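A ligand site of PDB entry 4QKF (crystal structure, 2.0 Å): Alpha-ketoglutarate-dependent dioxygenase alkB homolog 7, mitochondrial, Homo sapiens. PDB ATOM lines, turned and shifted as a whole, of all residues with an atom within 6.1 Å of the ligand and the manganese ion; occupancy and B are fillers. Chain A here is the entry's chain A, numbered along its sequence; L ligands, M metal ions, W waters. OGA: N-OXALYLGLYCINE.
OH of Tyr 150 lies within hydrogen-bond range of O4 of the ligand (2.6 Å). O3 of the ligand lies within salt-bridge range of NH1 of Arg 182, at 2.6 Å. OG of Ser 184 lies within hydrogen-bond range of O3 of the ligand, 2.6 Å away. The guanidinium group of Arg 188 lies within salt-bridge range of an oxygen (O1) of the ligand, 2.9 Å away.
The side-chain carboxylate (OD2) of Asp 108 is in salt-bridge range of the guanidinium group (NE) of Arg 188, 2.7 Å away. The backbone carbonyl oxygen of Gly 119 sits at hydrogen-bond distance from the backbone NH of Tyr 150 (2.9 Å). The guanidinium group (NH1) of Arg 182 is in hydrogen-bond range of the side-chain hydroxyl (OG) of Ser 184 (2.8 Å). The backbone carbonyl oxygen of Arg 182 sits at hydrogen-bond distance from the backbone NH of Leu 97 (2.8 Å). N of Ser 184 is in hydrogen-bond range of O of Leu 95 (2.7 Å). NH1 of Arg 188 is in hydrogen-bond range of ND1 of His 93. The backbone NH (N) of Ile 186 is in hydrogen-bond range of the backbone carbonyl oxygen (O) of His 93 (2.8 Å). N of Ile 103 sits at hydrogen-bond distance from O of Ile 164, at 3.0 Å.
His 93 touches the ligand. Leu 95 touches the ligand. Ile 164 touches the ligand (CD1 to C4, 3.5 Å). CD1 of Ile 186 touches N1 of the ligand (3.8 Å). Hydrophobic or aromatic side chains within 4 Å of the ligand: His 93, Leu 95, His 106, Tyr 150, His 162, Ile 164 and Ile 186. Within 4 Å of the ligand: His 93, Leu 95, His 106, Tyr 150, His 162, Ile 164, Arg 182, Ser 184, Ile 186 and Arg 188.
The nearest printed residue that does not touch the manganese ion is Arg 188 (4.2 Å).
OD1 of Asp 108 is bound to the manganese ion (2.3 Å). A ring nitrogen (NE2) of His 106 binds the manganese ion (2.4 Å). The manganese ion is bound by NE2 of His 162, at 2.4 Å. An oxygen (O2') of the ligand is bound to the manganese ion, at 2.4 Å. Slightly farther from the manganese ion lies an oxygen (O2) of the ligand (2.7 Å).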
ATOM      1  N   ALA A  54      17.307 -17.446  27.754  1.00  0.00           N
ATOM      2  CA  ALA A  54      16.030 -17.394  27.030  1.00  0.00           C
ATOM      3  C   ALA A  54      15.675 -18.753  26.392  1.00  0.00           C
ATOM      4  O   ALA A  54      14.544 -19.185  26.451  1.00  0.00           O
ATOM      5  CB  ALA A  54      16.105 -16.318  25.963  1.00  0.00           C
ATOM      6  N   ILE A  55      16.673 -19.428  25.850  1.00  0.00           N
ATOM      7  CA  ILE A  55      16.477 -20.669  25.103  1.00  0.00           C
ATOM      8  C   ILE A  55      16.932 -21.830  25.957  1.00  0.00           C
ATOM      9  O   ILE A  55      18.058 -21.795  26.498  1.00  0.00           O
ATOM     10  CB  ILE A  55      17.293 -20.656  23.806  1.00  0.00           C
ATOM     11  CG1 ILE A  55      17.211 -19.300  23.131  1.00  0.00           C
ATOM     12  CG2 ILE A  55      16.848 -21.760  22.854  1.00  0.00           C
ATOM     13  CD1 ILE A  55      18.283 -19.099  22.080  1.00  0.00           C
ATOM     14  N   HIS A  93      21.117 -17.071  11.800  1.00  0.00           N
ATOM     15  CA  HIS A  93      21.040 -17.836  13.028  1.00  0.00           C
ATOM     16  C   HIS A  93      20.139 -19.076  12.890  1.00  0.00           C
ATOM     17  O   HIS A  93      18.921 -18.989  12.630  1.00  0.00           O
ATOM     18  CB  HIS A  93      20.602 -16.891  14.164  1.00  0.00           C
ATOM     19  CG  HIS A  93      20.204 -17.598  15.403  1.00  0.00           C
ATOM     20  ND1 HIS A  93      19.186 -17.154  16.228  1.00  0.00           N
ATOM     21  CD2 HIS A  93      20.686 -18.722  15.980  1.00  0.00           C
ATOM     22  CE1 HIS A  93      19.043 -17.985  17.230  1.00  0.00           C
ATOM     23  NE2 HIS A  93      19.941 -18.941  17.107  1.00  0.00           N
ATOM     24  N   LEU A  95      18.626 -22.223  14.696  1.00  0.00           N
ATOM     25  CA  LEU A  95      18.324 -22.697  16.009  1.00  0.00           C
ATOM     26  C   LEU A  95      17.572 -24.031  16.033  1.00  0.00           C
ATOM     27  O   LEU A  95      16.441 -24.122  15.522  1.00  0.00           O
ATOM     28  CB  LEU A  95      17.478 -21.631  16.700  1.00  0.00           C
ATOM     29  CG  LEU A  95      17.080 -21.916  18.117  1.00  0.00           C
ATOM     30  CD1 LEU A  95      18.299 -22.194  18.988  1.00  0.00           C
ATOM     31  CD2 LEU A  95      16.298 -20.722  18.651  1.00  0.00           C
ATOM     32  N   LEU A  97      15.697 -26.638  18.252  1.00  0.00           N
ATOM     33  CA  LEU A  97      15.077 -26.953  19.539  1.00  0.00           C
ATOM     34  C   LEU A  97      14.688 -28.415  19.595  1.00  0.00           C
ATOM     35  O   LEU A  97      14.102 -28.975  18.658  1.00  0.00           O
ATOM     36  CB  LEU A  97      13.848 -26.089  19.839  1.00  0.00           C
ATOM     37  CG  LEU A  97      14.030 -24.636  20.314  1.00  0.00           C
ATOM     38  CD1 LEU A  97      12.688 -24.073  20.725  1.00  0.00           C
ATOM     39  CD2 LEU A  97      15.060 -24.447  21.452  1.00  0.00           C
ATOM     40  N   ILE A 103      11.516 -21.718  24.360  1.00  0.00           N
ATOM     41  CA  ILE A 103      12.061 -20.378  24.407  1.00  0.00           C
ATOM     42  C   ILE A 103      11.199 -19.497  25.296  1.00  0.00           C
ATOM     43  O   ILE A 103       9.967 -19.409  25.138  1.00  0.00           O
ATOM     44  CB  ILE A 103      12.199 -19.788  22.993  1.00  0.00           C
ATOM     45  CG1 ILE A 103      12.959 -20.764  22.105  1.00  0.00           C
ATOM     46  CG2 ILE A 103      12.881 -18.443  23.062  1.00  0.00           C
ATOM     47  CD1 ILE A 103      13.509 -20.208  20.808  1.00  0.00           C
ATOM     48  N   HIS A 106      11.145 -12.971  25.496  1.00  0.00           N
ATOM     49  CA  HIS A 106      12.207 -11.981  25.404  1.00  0.00           C
ATOM     50  C   HIS A 106      12.052 -11.102  24.220  1.00  0.00           C
ATOM     51  O   HIS A 106      11.359 -11.411  23.256  1.00  0.00           O
ATOM     52  CB  HIS A 106      13.538 -12.669  25.237  1.00  0.00           C
ATOM     53  CG  HIS A 106      13.548 -13.586  24.065  1.00  0.00           C
ATOM     54  ND1 HIS A 106      12.772 -14.718  24.014  1.00  0.00           N
ATOM     55  CD2 HIS A 106      14.202 -13.512  22.889  1.00  0.00           C
ATOM     56  CE1 HIS A 106      12.958 -15.325  22.859  1.00  0.00           C
ATOM     57  NE2 HIS A 106      13.792 -14.595  22.140  1.00  0.00           N
ATOM     58  N   VAL A 107      12.784 -10.009  24.253  1.00  0.00           N
ATOM     59  CA  VAL A 107      12.910  -9.182  23.096  1.00  0.00           C
ATOM     60  C   VAL A 107      14.334  -9.366  22.614  1.00  0.00           C
ATOM     61  O   VAL A 107      15.247  -9.447  23.424  1.00  0.00           O
ATOM     62  CB  VAL A 107      12.591  -7.733  23.477  1.00  0.00           C
ATOM     63  CG1 VAL A 107      12.933  -6.805  22.339  1.00  0.00           C
ATOM     64  CG2 VAL A 107      11.104  -7.631  23.850  1.00  0.00           C
ATOM     65  N   ASP A 108      14.530  -9.356  21.301  1.00  0.00           N
ATOM     66  CA  ASP A 108      15.835  -9.481  20.718  1.00  0.00           C
ATOM     67  C   ASP A 108      16.650  -8.235  20.933  1.00  0.00           C
ATOM     68  O   ASP A 108      16.136  -7.132  20.775  1.00  0.00           O
ATOM     69  CB  ASP A 108      15.764  -9.690  19.215  1.00  0.00           C
ATOM     70  CG  ASP A 108      15.567 -11.111  18.855  1.00  0.00           C
ATOM     71  OD1 ASP A 108      15.002 -11.826  19.675  1.00  0.00           O
ATOM     72  OD2 ASP A 108      15.940 -11.526  17.757  1.00  0.00           O
ATOM     73  N   ILE A 117      12.714  -9.049  12.414  1.00  0.00           N
ATOM     74  CA  ILE A 117      13.097 -10.435  12.626  1.00  0.00           C
ATOM     75  C   ILE A 117      12.201 -11.322  11.745  1.00  0.00           C
ATOM     76  O   ILE A 117      10.977 -11.182  11.760  1.00  0.00           O
ATOM     77  CB  ILE A 117      12.918 -10.819  14.090  1.00  0.00           C
ATOM     78  CG1 ILE A 117      13.871 -10.014  14.997  1.00  0.00           C
ATOM     79  CG2 ILE A 117      13.165 -12.299  14.274  1.00  0.00           C
ATOM     80  CD1 ILE A 117      13.360  -9.817  16.371  1.00  0.00           C
ATOM     81  N   GLY A 119      11.625 -15.481  10.913  1.00  0.00           N
ATOM     82  CA  GLY A 119      11.974 -16.874  11.084  1.00  0.00           C
ATOM     83  C   GLY A 119      11.244 -17.841  10.166  1.00  0.00           C
ATOM     84  O   GLY A 119      10.016 -17.767  10.027  1.00  0.00           O
ATOM     85  N   LEU A 120      12.011 -18.761   9.559  1.00  0.00           N
ATOM     86  CA  LEU A 120      11.452 -19.977   8.955  1.00  0.00           C
ATOM     87  C   LEU A 120      11.360 -21.089   9.951  1.00  0.00           C
ATOM     88  O   LEU A 120      12.226 -21.233  10.830  1.00  0.00           O
ATOM     89  CB  LEU A 120      12.297 -20.404   7.736  1.00  0.00           C
ATOM     90  CG  LEU A 120      12.356 -19.346   6.664  1.00  0.00           C
ATOM     91  CD1 LEU A 120      13.417 -19.615   5.597  1.00  0.00           C
ATOM     92  CD2 LEU A 120      10.989 -19.219   6.013  1.00  0.00           C
ATOM     93  N   MET A 128       4.265 -19.448  18.780  1.00  0.00           N
ATOM     94  CA  MET A 128       4.998 -18.300  19.354  1.00  0.00           C
ATOM     95  C   MET A 128       4.023 -17.302  20.015  1.00  0.00           C
ATOM     96  O   MET A 128       3.082 -16.820  19.372  1.00  0.00           O
ATOM     97  CB  MET A 128       5.757 -17.611  18.253  1.00  0.00           C
ATOM     98  CG  MET A 128       6.194 -16.197  18.562  1.00  0.00           C
ATOM     99  SD  MET A 128       7.138 -15.590  17.200  1.00  0.00           S
ATOM    100  CE  MET A 128       8.535 -16.710  17.193  1.00  0.00           C
ATOM    101  N   TYR A 150       7.472 -16.437   9.699  1.00  0.00           N
ATOM    102  CA  TYR A 150       6.929 -15.288  10.460  1.00  0.00           C
ATOM    103  C   TYR A 150       7.842 -14.097  10.278  1.00  0.00           C
ATOM    104  O   TYR A 150       9.040 -14.251   9.960  1.00  0.00           O
ATOM    105  CB  TYR A 150       6.679 -15.584  11.937  1.00  0.00           C
ATOM    106  CG  TYR A 150       7.911 -15.801  12.775  1.00  0.00           C
ATOM    107  CD1 TYR A 150       8.621 -14.736  13.319  1.00  0.00           C
ATOM    108  CD2 TYR A 150       8.394 -17.090  13.018  1.00  0.00           C
ATOM    109  CE1 TYR A 150       9.758 -14.937  14.088  1.00  0.00           C
ATOM    110  CE2 TYR A 150       9.543 -17.308  13.791  1.00  0.00           C
ATOM    111  CZ  TYR A 150      10.213 -16.225  14.321  1.00  0.00           C
ATOM    112  OH  TYR A 150      11.371 -16.416  15.093  1.00  0.00           O
ATOM    113  N   HIS A 162       8.479 -12.212  22.888  1.00  0.00           N
ATOM    114  CA  HIS A 162       8.031 -13.342  22.161  1.00  0.00           C
ATOM    115  C   HIS A 162       8.774 -14.601  22.606  1.00  0.00           C
ATOM    116  O   HIS A 162       9.940 -14.545  23.057  1.00  0.00           O
ATOM    117  CB  HIS A 162       8.212 -13.069  20.688  1.00  0.00           C
ATOM    118  CG  HIS A 162       9.634 -13.029  20.264  1.00  0.00           C
ATOM    119  ND1 HIS A 162      10.251 -11.890  19.807  1.00  0.00           N
ATOM    120  CD2 HIS A 162      10.566 -14.014  20.222  1.00  0.00           C
ATOM    121  CE1 HIS A 162      11.500 -12.178  19.482  1.00  0.00           C
ATOM    122  NE2 HIS A 162      11.706 -13.460  19.705  1.00  0.00           N
ATOM    123  N   GLU A 163       8.079 -15.715  22.503  1.00  0.00           N
ATOM    124  CA  GLU A 163       8.495 -16.988  23.096  1.00  0.00           C
ATOM    125  C   GLU A 163       7.917 -18.136  22.279  1.00  0.00           C
ATOM    126  O   GLU A 163       6.877 -17.965  21.632  1.00  0.00           O
ATOM    127  CB  GLU A 163       7.996 -17.073  24.523  1.00  0.00           C
ATOM    128  CG  GLU A 163       6.495 -17.142  24.642  1.00  0.00           C
ATOM    129  CD  GLU A 163       6.003 -16.833  26.017  1.00  0.00           C
ATOM    130  OE1 GLU A 163       5.949 -17.742  26.871  1.00  0.00           O
ATOM    131  OE2 GLU A 163       5.658 -15.651  26.229  1.00  0.00           O
ATOM    132  N   ILE A 164       8.574 -19.294  22.302  1.00  0.00           N
ATOM    133  CA  ILE A 164       8.053 -20.508  21.673  1.00  0.00           C
ATOM    134  C   ILE A 164       7.712 -21.452  22.788  1.00  0.00           C
ATOM    135  O   ILE A 164       8.585 -21.832  23.573  1.00  0.00           O
ATOM    136  CB  ILE A 164       9.063 -21.184  20.717  1.00  0.00           C
ATOM    137  CG1 ILE A 164       9.280 -20.336  19.473  1.00  0.00           C
ATOM    138  CG2 ILE A 164       8.547 -22.545  20.271  1.00  0.00           C
ATOM    139  CD1 ILE A 164      10.232 -19.161  19.651  1.00  0.00           C
ATOM    140  N   ARG A 182      12.350 -28.978  16.395  1.00  0.00           N
ATOM    141  CA  ARG A 182      12.015 -27.946  15.432  1.00  0.00           C
ATOM    142  C   ARG A 182      13.262 -27.136  15.191  1.00  0.00           C
ATOM    143  O   ARG A 182      13.881 -26.638  16.122  1.00  0.00           O
ATOM    144  CB  ARG A 182      10.924 -26.999  15.985  1.00  0.00           C
ATOM    145  CG  ARG A 182      10.975 -25.582  15.412  1.00  0.00           C
ATOM    146  CD  ARG A 182      10.148 -24.589  16.241  1.00  0.00           C
ATOM    147  NE  ARG A 182       9.894 -23.356  15.496  1.00  0.00           N
ATOM    148  CZ  ARG A 182      10.577 -22.224  15.593  1.00  0.00           C
ATOM    149  NH1 ARG A 182      11.626 -22.107  16.428  1.00  0.00           N
ATOM    150  NH2 ARG A 182      10.238 -21.196  14.815  1.00  0.00           N
ATOM    151  N   ILE A 183      13.613 -26.985  13.934  1.00  0.00           N
ATOM    152  CA  ILE A 183      14.697 -26.111  13.578  1.00  0.00           C
ATOM    153  C   ILE A 183      14.110 -24.773  13.121  1.00  0.00           C
ATOM    154  O   ILE A 183      13.085 -24.756  12.436  1.00  0.00           O
ATOM    155  CB  ILE A 183      15.602 -26.732  12.517  1.00  0.00           C
ATOM    156  CG1 ILE A 183      16.131 -28.104  12.995  1.00  0.00           C
ATOM    157  CG2 ILE A 183      16.768 -25.821  12.218  1.00  0.00           C
ATOM    158  CD1 ILE A 183      16.846 -28.907  11.921  1.00  0.00           C
ATOM    159  N   SER A 184      14.758 -23.689  13.519  1.00  0.00           N
ATOM    160  CA  SER A 184      14.437 -22.342  13.045  1.00  0.00           C
ATOM    161  C   SER A 184      15.610 -21.810  12.277  1.00  0.00           C
ATOM    162  O   SER A 184      16.778 -21.979  12.670  1.00  0.00           O
ATOM    163  CB  SER A 184      14.166 -21.378  14.203  1.00  0.00           C
ATOM    164  OG  SER A 184      14.261 -22.022  15.469  1.00  0.00           O
ATOM    165  N   VAL A 185      15.306 -21.141  11.181  1.00  0.00           N
ATOM    166  CA  VAL A 185      16.301 -20.415  10.430  1.00  0.00           C
ATOM    167  C   VAL A 185      15.898 -18.965  10.511  1.00  0.00           C
ATOM    168  O   VAL A 185      14.855 -18.575   9.943  1.00  0.00           O
ATOM    169  CB  VAL A 185      16.307 -20.873   8.978  1.00  0.00           C
ATOM    170  CG1 VAL A 185      17.337 -20.116   8.173  1.00  0.00           C
ATOM    171  CG2 VAL A 185      16.558 -22.381   8.921  1.00  0.00           C
ATOM    172  N   ILE A 186      16.697 -18.175  11.229  1.00  0.00           N
ATOM    173  CA  ILE A 186      16.319 -16.782  11.489  1.00  0.00           C
ATOM    174  C   ILE A 186      17.220 -15.745  10.817  1.00  0.00           C
ATOM    175  O   ILE A 186      18.461 -15.812  10.866  1.00  0.00           O
ATOM    176  CB  ILE A 186      16.192 -16.522  12.997  1.00  0.00           C
ATOM    177  CG1 ILE A 186      15.747 -15.078  13.287  1.00  0.00           C
ATOM    178  CG2 ILE A 186      17.500 -16.753  13.719  1.00  0.00           C
ATOM    179  CD1 ILE A 186      14.881 -15.050  14.509  1.00  0.00           C
ATOM    180  N   ARG A 188      18.078 -11.648  10.427  1.00  0.00           N
ATOM    181  CA  ARG A 188      17.889 -10.418  11.195  1.00  0.00           C
ATOM    182  C   ARG A 188      18.448  -9.216  10.474  1.00  0.00           C
ATOM    183  O   ARG A 188      19.301  -9.333   9.616  1.00  0.00           O
ATOM    184  CB  ARG A 188      18.450 -10.578  12.622  1.00  0.00           C
ATOM    185  CG  ARG A 188      17.634 -11.405  13.575  1.00  0.00           C
ATOM    186  CD  ARG A 188      18.401 -11.604  14.875  1.00  0.00           C
ATOM    187  NE  ARG A 188      17.688 -12.340  15.891  1.00  0.00           N
ATOM    188  CZ  ARG A 188      17.862 -13.623  16.191  1.00  0.00           C
ATOM    189  NH1 ARG A 188      18.728 -14.376  15.524  1.00  0.00           N
ATOM    190  NH2 ARG A 188      17.145 -14.162  17.146  1.00  0.00           N
HETATM  191  C1  OGA L   1      15.448 -16.329  19.324  1.00  0.00           C
HETATM  192  C2  OGA L   1      14.062 -16.372  18.852  1.00  0.00           C
HETATM  193  C4  OGA L   1      12.680 -17.783  17.482  1.00  0.00           C
HETATM  194  C5  OGA L   1      12.977 -18.795  16.385  1.00  0.00           C
HETATM  195  O1  OGA L   1      16.383 -16.618  18.585  1.00  0.00           O
HETATM  196  O2  OGA L   1      15.694 -16.004  20.486  1.00  0.00           O
HETATM  197  O2' OGA L   1      13.193 -16.128  19.670  1.00  0.00           O
HETATM  198  O3  OGA L   1      13.164 -19.984  16.740  1.00  0.00           O
HETATM  199  N1  OGA L   1      13.796 -16.878  17.643  1.00  0.00           N
HETATM  200  O4  OGA L   1      13.082 -18.413  15.186  1.00  0.00           O
HETATM  201 MN    MN M   1      14.031 -13.899  19.886  1.00  0.00          MN
HETATM  202  O   HOH W   1      16.949 -14.053  21.597  1.00  0.00           O
